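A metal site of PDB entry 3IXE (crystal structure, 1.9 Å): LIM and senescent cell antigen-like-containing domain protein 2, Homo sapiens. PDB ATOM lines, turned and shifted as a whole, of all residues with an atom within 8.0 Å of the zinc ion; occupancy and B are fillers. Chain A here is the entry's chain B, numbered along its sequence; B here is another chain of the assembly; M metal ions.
SG of Cys 14 sits close to N of Arg 16. N of Cys 14 lies within hydrogen-bond range of O of Ala 19, at 3.0 Å. A ring nitrogen (NE2) of His 36 lies within hydrogen-bond range of the backbone carbonyl oxygen (O) of Arg 20 (2.7 Å). The side-chain sulfur (SG) of Cys 39 lies close to a ring nitrogen (NE2) of His 38, 3.7 Å away. SG of Cys 39 sits close to NE of Arg 16, at 3.3 Å. N of Ala 19 sits close to SG of Cys 17 (3.5 Å). O of Cys 17 is in hydrogen-bond range of NZ of Lys 146 of chain B (2.7 Å).
The zinc ion is bound by SG of Cys 14 (2.3 Å), ND1 of His 36 (2.3 Å), SG of Cys 39 (2.3 Å) and SG of Cys 17 (2.3 Å). The zinc ion has four donor atoms within binding distance.
Four residues have an atom within 4 Å of the zinc ion: Cys 14, Cys 17, His 36 and Cys 39. The nearest printed residue that does not touch the zinc ion is His 38 (4.7 Å).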
ATOM      1  N   VAL A  13     -18.604  -2.663 -30.012  1.00  0.00           N
ATOM      2  CA  VAL A  13     -17.917  -2.894 -28.736  1.00  0.00           C
ATOM      3  C   VAL A  13     -18.806  -2.485 -27.557  1.00  0.00           C
ATOM      4  O   VAL A  13     -19.796  -1.760 -27.723  1.00  0.00           O
ATOM      5  CB  VAL A  13     -16.539  -2.181 -28.636  1.00  0.00           C
ATOM      6  CG1 VAL A  13     -15.587  -2.679 -29.742  1.00  0.00           C
ATOM      7  CG2 VAL A  13     -16.687  -0.657 -28.672  1.00  0.00           C
ATOM      8  N   CYS A  14     -18.445  -2.960 -26.368  1.00  0.00           N
ATOM      9  CA  CYS A  14     -19.185  -2.665 -25.144  1.00  0.00           C
ATOM     10  C   CYS A  14     -19.006  -1.218 -24.729  1.00  0.00           C
ATOM     11  O   CYS A  14     -17.891  -0.712 -24.641  1.00  0.00           O
ATOM     12  CB  CYS A  14     -18.740  -3.599 -24.026  1.00  0.00           C
ATOM     13  SG  CYS A  14     -19.480  -3.234 -22.409  1.00  0.00           S
ATOM     14  N   GLN A  15     -20.132  -0.544 -24.484  1.00  0.00           N
ATOM     15  CA  GLN A  15     -20.148   0.836 -24.019  1.00  0.00           C
ATOM     16  C   GLN A  15     -19.262   1.048 -22.770  1.00  0.00           C
ATOM     17  O   GLN A  15     -18.526   2.027 -22.668  1.00  0.00           O
ATOM     18  CB  GLN A  15     -21.589   1.246 -23.701  1.00  0.00           C
ATOM     19  CG  GLN A  15     -21.788   2.704 -23.311  1.00  0.00           C
ATOM     20  CD  GLN A  15     -21.776   3.624 -24.491  1.00  0.00           C
ATOM     21  OE1 GLN A  15     -22.484   3.413 -25.481  1.00  0.00           O
ATOM     22  NE2 GLN A  15     -20.971   4.680 -24.404  1.00  0.00           N
ATOM     23  N   ARG A  16     -19.331   0.103 -21.840  1.00  0.00           N
ATOM     24  CA  ARG A  16     -18.671   0.256 -20.544  1.00  0.00           C
ATOM     25  C   ARG A  16     -17.172  -0.048 -20.592  1.00  0.00           C
ATOM     26  O   ARG A  16     -16.361   0.722 -20.057  1.00  0.00           O
ATOM     27  CB  ARG A  16     -19.350  -0.615 -19.482  1.00  0.00           C
ATOM     28  CG  ARG A  16     -18.980  -0.225 -18.057  1.00  0.00           C
ATOM     29  CD  ARG A  16     -19.294  -1.337 -17.049  1.00  0.00           C
ATOM     30  NE  ARG A  16     -18.411  -2.495 -17.180  1.00  0.00           N
ATOM     31  CZ  ARG A  16     -17.164  -2.561 -16.713  1.00  0.00           C
ATOM     32  NH1 ARG A  16     -16.620  -1.529 -16.086  1.00  0.00           N
ATOM     33  NH2 ARG A  16     -16.461  -3.669 -16.882  1.00  0.00           N
ATOM     34  N   CYS A  17     -16.806  -1.177 -21.213  1.00  0.00           N
ATOM     35  CA  CYS A  17     -15.427  -1.691 -21.127  1.00  0.00           C
ATOM     36  C   CYS A  17     -14.625  -1.622 -22.433  1.00  0.00           C
ATOM     37  O   CYS A  17     -13.418  -1.868 -22.414  1.00  0.00           O
ATOM     38  CB  CYS A  17     -15.422  -3.119 -20.585  1.00  0.00           C
ATOM     39  SG  CYS A  17     -15.931  -4.375 -21.786  1.00  0.00           S
ATOM     40  N   GLN A  18     -15.306  -1.294 -23.526  1.00  0.00           N
ATOM     41  CA  GLN A  18     -14.682  -1.120 -24.856  1.00  0.00           C
ATOM     42  C   GLN A  18     -14.139  -2.410 -25.467  1.00  0.00           C
ATOM     43  O   GLN A  18     -13.483  -2.383 -26.511  1.00  0.00           O
ATOM     44  CB  GLN A  18     -13.599  -0.021 -24.836  1.00  0.00           C
ATOM     45  CG  GLN A  18     -14.138   1.391 -24.591  1.00  0.00           C
ATOM     46  CD  GLN A  18     -14.414   1.676 -23.131  1.00  0.00           C
ATOM     47  OE1 GLN A  18     -13.596   1.370 -22.259  1.00  0.00           O
ATOM     48  NE2 GLN A  18     -15.567   2.271 -22.853  1.00  0.00           N
ATOM     49  N   ALA A  19     -14.411  -3.550 -24.809  1.00  0.00           N
ATOM     50  CA  ALA A  19     -14.027  -4.845 -25.365  1.00  0.00           C
ATOM     51  C   ALA A  19     -15.044  -5.302 -26.402  1.00  0.00           C
ATOM     52  O   ALA A  19     -16.203  -4.879 -26.373  1.00  0.00           O
ATOM     53  CB  ALA A  19     -13.873  -5.889 -24.262  1.00  0.00           C
ATOM     54  N   ARG A  20     -14.609  -6.167 -27.317  1.00  0.00           N
ATOM     55  CA  ARG A  20     -15.456  -6.684 -28.384  1.00  0.00           C
ATOM     56  C   ARG A  20     -16.453  -7.739 -27.884  1.00  0.00           C
ATOM     57  O   ARG A  20     -16.415  -8.154 -26.715  1.00  0.00           O
ATOM     58  CB  ARG A  20     -14.591  -7.269 -29.503  1.00  0.00           C
ATOM     59  CG  ARG A  20     -13.847  -6.214 -30.314  1.00  0.00           C
ATOM     60  CD  ARG A  20     -12.638  -6.800 -31.051  1.00  0.00           C
ATOM     61  NE  ARG A  20     -11.586  -7.233 -30.140  1.00  0.00           N
ATOM     62  CZ  ARG A  20     -11.050  -8.446 -30.132  1.00  0.00           C
ATOM     63  NH1 ARG A  20     -11.461  -9.372 -30.993  1.00  0.00           N
ATOM     64  NH2 ARG A  20     -10.080  -8.746 -29.275  1.00  0.00           N
ATOM     65  N   PHE A  21     -17.343  -8.153 -28.788  1.00  0.00           N
ATOM     66  CA  PHE A  21     -18.324  -9.198 -28.512  1.00  0.00           C
ATOM     67  C   PHE A  21     -17.987 -10.471 -29.276  1.00  0.00           C
ATOM     68  O   PHE A  21     -17.664 -10.414 -30.461  1.00  0.00           O
ATOM     69  CB  PHE A  21     -19.728  -8.745 -28.927  1.00  0.00           C
ATOM     70  CG  PHE A  21     -20.214  -7.533 -28.193  1.00  0.00           C
ATOM     71  CD1 PHE A  21     -20.572  -7.596 -26.847  1.00  0.00           C
ATOM     72  CD2 PHE A  21     -20.343  -6.323 -28.862  1.00  0.00           C
ATOM     73  CE1 PHE A  21     -21.035  -6.462 -26.180  1.00  0.00           C
ATOM     74  CE2 PHE A  21     -20.813  -5.184 -28.199  1.00  0.00           C
ATOM     75  CZ  PHE A  21     -21.157  -5.267 -26.855  1.00  0.00           C
ATOM     76  N   GLU A  25     -22.446 -14.542 -27.730  1.00  0.00           N
ATOM     77  CA  GLU A  25     -23.013 -13.904 -26.530  1.00  0.00           C
ATOM     78  C   GLU A  25     -24.127 -12.909 -26.852  1.00  0.00           C
ATOM     79  O   GLU A  25     -24.124 -12.273 -27.905  1.00  0.00           O
ATOM     80  CB  GLU A  25     -21.922 -13.241 -25.690  1.00  0.00           C
ATOM     81  CG  GLU A  25     -21.285 -12.013 -26.330  1.00  0.00           C
ATOM     82  CD  GLU A  25     -20.225 -11.382 -25.444  1.00  0.00           C
ATOM     83  OE1 GLU A  25     -20.545 -11.070 -24.268  1.00  0.00           O
ATOM     84  OE2 GLU A  25     -19.081 -11.202 -25.917  1.00  0.00           O
ATOM     85  N   LEU A  34     -24.721  -0.624 -26.378  1.00  0.00           N
ATOM     86  CA  LEU A  34     -24.440  -2.052 -26.334  1.00  0.00           C
ATOM     87  C   LEU A  34     -23.547  -2.384 -25.133  1.00  0.00           C
ATOM     88  O   LEU A  34     -22.592  -1.674 -24.857  1.00  0.00           O
ATOM     89  CB  LEU A  34     -23.780  -2.515 -27.631  1.00  0.00           C
ATOM     90  CG  LEU A  34     -24.479  -2.259 -28.982  1.00  0.00           C
ATOM     91  CD1 LEU A  34     -24.162  -0.868 -29.495  1.00  0.00           C
ATOM     92  CD2 LEU A  34     -24.064  -3.298 -30.021  1.00  0.00           C
ATOM     93  N   TYR A  35     -23.895  -3.472 -24.437  1.00  0.00           N
ATOM     94  CA  TYR A  35     -23.169  -3.915 -23.244  1.00  0.00           C
ATOM     95  C   TYR A  35     -22.983  -5.428 -23.194  1.00  0.00           C
ATOM     96  O   TYR A  35     -23.900  -6.187 -23.556  1.00  0.00           O
ATOM     97  CB  TYR A  35     -23.926  -3.509 -21.978  1.00  0.00           C
ATOM     98  CG  TYR A  35     -24.056  -2.032 -21.727  1.00  0.00           C
ATOM     99  CD1 TYR A  35     -23.035  -1.324 -21.075  1.00  0.00           C
ATOM    100  CD2 TYR A  35     -25.189  -1.332 -22.122  1.00  0.00           C
ATOM    101  CE1 TYR A  35     -23.153   0.030 -20.823  1.00  0.00           C
ATOM    102  CE2 TYR A  35     -25.322   0.032 -21.878  1.00  0.00           C
ATOM    103  CZ  TYR A  35     -24.292   0.711 -21.228  1.00  0.00           C
ATOM    104  OH  TYR A  35     -24.387   2.053 -20.986  1.00  0.00           O
ATOM    105  N   HIS A  36     -21.830  -5.871 -22.698  1.00  0.00           N
ATOM    106  CA  HIS A  36     -21.710  -7.244 -22.216  1.00  0.00           C
ATOM    107  C   HIS A  36     -22.708  -7.430 -21.071  1.00  0.00           C
ATOM    108  O   HIS A  36     -22.939  -6.497 -20.300  1.00  0.00           O
ATOM    109  CB  HIS A  36     -20.297  -7.517 -21.672  1.00  0.00           C
ATOM    110  CG  HIS A  36     -19.237  -7.514 -22.732  1.00  0.00           C
ATOM    111  ND1 HIS A  36     -18.251  -6.549 -22.787  1.00  0.00           N
ATOM    112  CD2 HIS A  36     -19.007  -8.354 -23.768  1.00  0.00           C
ATOM    113  CE1 HIS A  36     -17.458  -6.801 -23.809  1.00  0.00           C
ATOM    114  NE2 HIS A  36     -17.896  -7.883 -24.429  1.00  0.00           N
ATOM    115  N   GLU A  37     -23.305  -8.622 -20.975  1.00  0.00           N
ATOM    116  CA  GLU A  37     -24.229  -8.951 -19.876  1.00  0.00           C
ATOM    117  C   GLU A  37     -23.620  -8.587 -18.523  1.00  0.00           C
ATOM    118  O   GLU A  37     -24.281  -7.992 -17.672  1.00  0.00           O
ATOM    119  CB  GLU A  37     -24.623 -10.434 -19.905  1.00  0.00           C
ATOM    120  CG  GLU A  37     -25.742 -10.802 -18.924  1.00  0.00           C
ATOM    121  CD  GLU A  37     -26.261 -12.224 -19.089  1.00  0.00           C
ATOM    122  OE1 GLU A  37     -27.472 -12.438 -18.856  1.00  0.00           O
ATOM    123  OE2 GLU A  37     -25.482 -13.141 -19.430  1.00  0.00           O
ATOM    124  N   HIS A  38     -22.339  -8.949 -18.336  1.00  0.00           N
ATOM    125  CA  HIS A  38     -21.663  -8.710 -17.069  1.00  0.00           C
ATOM    126  C   HIS A  38     -21.230  -7.251 -16.890  1.00  0.00           C
ATOM    127  O   HIS A  38     -20.690  -6.879 -15.850  1.00  0.00           O
ATOM    128  CB  HIS A  38     -20.477  -9.655 -16.878  1.00  0.00           C
ATOM    129  CG  HIS A  38     -19.301  -9.351 -17.771  1.00  0.00           C
ATOM    130  ND1 HIS A  38     -19.082 -10.021 -18.957  1.00  0.00           N
ATOM    131  CD2 HIS A  38     -18.287  -8.477 -17.638  1.00  0.00           C
ATOM    132  CE1 HIS A  38     -17.993  -9.546 -19.518  1.00  0.00           C
ATOM    133  NE2 HIS A  38     -17.484  -8.612 -18.739  1.00  0.00           N
ATOM    134  N   CYS A  39     -21.488  -6.433 -17.913  1.00  0.00           N
ATOM    135  CA  CYS A  39     -21.181  -5.016 -17.867  1.00  0.00           C
ATOM    136  C   CYS A  39     -22.427  -4.143 -17.646  1.00  0.00           C
ATOM    137  O   CYS A  39     -22.317  -3.022 -17.167  1.00  0.00           O
ATOM    138  CB  CYS A  39     -20.444  -4.588 -19.134  1.00  0.00           C
ATOM    139  SG  CYS A  39     -18.721  -5.150 -19.183  1.00  0.00           S
ATOM    140  N   PHE A  40     -23.599  -4.663 -17.995  1.00  0.00           N
ATOM    141  CA  PHE A  40     -24.857  -3.977 -17.675  1.00  0.00           C
ATOM    142  C   PHE A  40     -25.299  -4.368 -16.260  1.00  0.00           C
ATOM    143  O   PHE A  40     -26.268  -5.112 -16.068  1.00  0.00           O
ATOM    144  CB  PHE A  40     -25.937  -4.245 -18.734  1.00  0.00           C
ATOM    145  CG  PHE A  40     -27.137  -3.343 -18.619  1.00  0.00           C
ATOM    146  CD1 PHE A  40     -27.019  -1.976 -18.871  1.00  0.00           C
ATOM    147  CD2 PHE A  40     -28.379  -3.861 -18.266  1.00  0.00           C
ATOM    148  CE1 PHE A  40     -28.131  -1.137 -18.754  1.00  0.00           C
ATOM    149  CE2 PHE A  40     -29.500  -3.027 -18.163  1.00  0.00           C
ATOM    150  CZ  PHE A  40     -29.374  -1.665 -18.412  1.00  0.00           C
ATOM    151  N   PHE B 114     -12.544  -3.858 -12.277  1.00  0.00           N
ATOM    152  CA  PHE B 114     -13.819  -3.651 -12.974  1.00  0.00           C
ATOM    153  C   PHE B 114     -13.716  -2.510 -13.985  1.00  0.00           C
ATOM    154  O   PHE B 114     -14.239  -2.608 -15.101  1.00  0.00           O
ATOM    155  CB  PHE B 114     -14.945  -3.392 -11.968  1.00  0.00           C
ATOM    156  CG  PHE B 114     -16.328  -3.290 -12.606  1.00  0.00           C
ATOM    157  CD1 PHE B 114     -16.899  -4.385 -13.256  1.00  0.00           C
ATOM    158  CD2 PHE B 114     -17.069  -2.106 -12.519  1.00  0.00           C
ATOM    159  CE1 PHE B 114     -18.176  -4.305 -13.825  1.00  0.00           C
ATOM    160  CE2 PHE B 114     -18.342  -2.014 -13.110  1.00  0.00           C
ATOM    161  CZ  PHE B 114     -18.888  -3.114 -13.738  1.00  0.00           C
ATOM    162  N   LYS B 146     -10.690  -7.781 -17.197  1.00  0.00           N
ATOM    163  CA  LYS B 146     -10.543  -8.447 -18.489  1.00  0.00           C
ATOM    164  C   LYS B 146      -9.405  -9.449 -18.375  1.00  0.00           C
ATOM    165  O   LYS B 146      -8.494  -9.259 -17.559  1.00  0.00           O
ATOM    166  CB  LYS B 146     -10.229  -7.431 -19.591  1.00  0.00           C
ATOM    167  CG  LYS B 146     -11.351  -6.507 -19.960  1.00  0.00           C
ATOM    168  CD  LYS B 146     -10.768  -5.310 -20.684  1.00  0.00           C
ATOM    169  CE  LYS B 146     -11.842  -4.460 -21.317  1.00  0.00           C
ATOM    170  NZ  LYS B 146     -11.191  -3.358 -22.064  1.00  0.00           N
HETATM  171 ZN    ZN M   1     -18.152  -4.764 -21.364  1.00  0.00          ZN
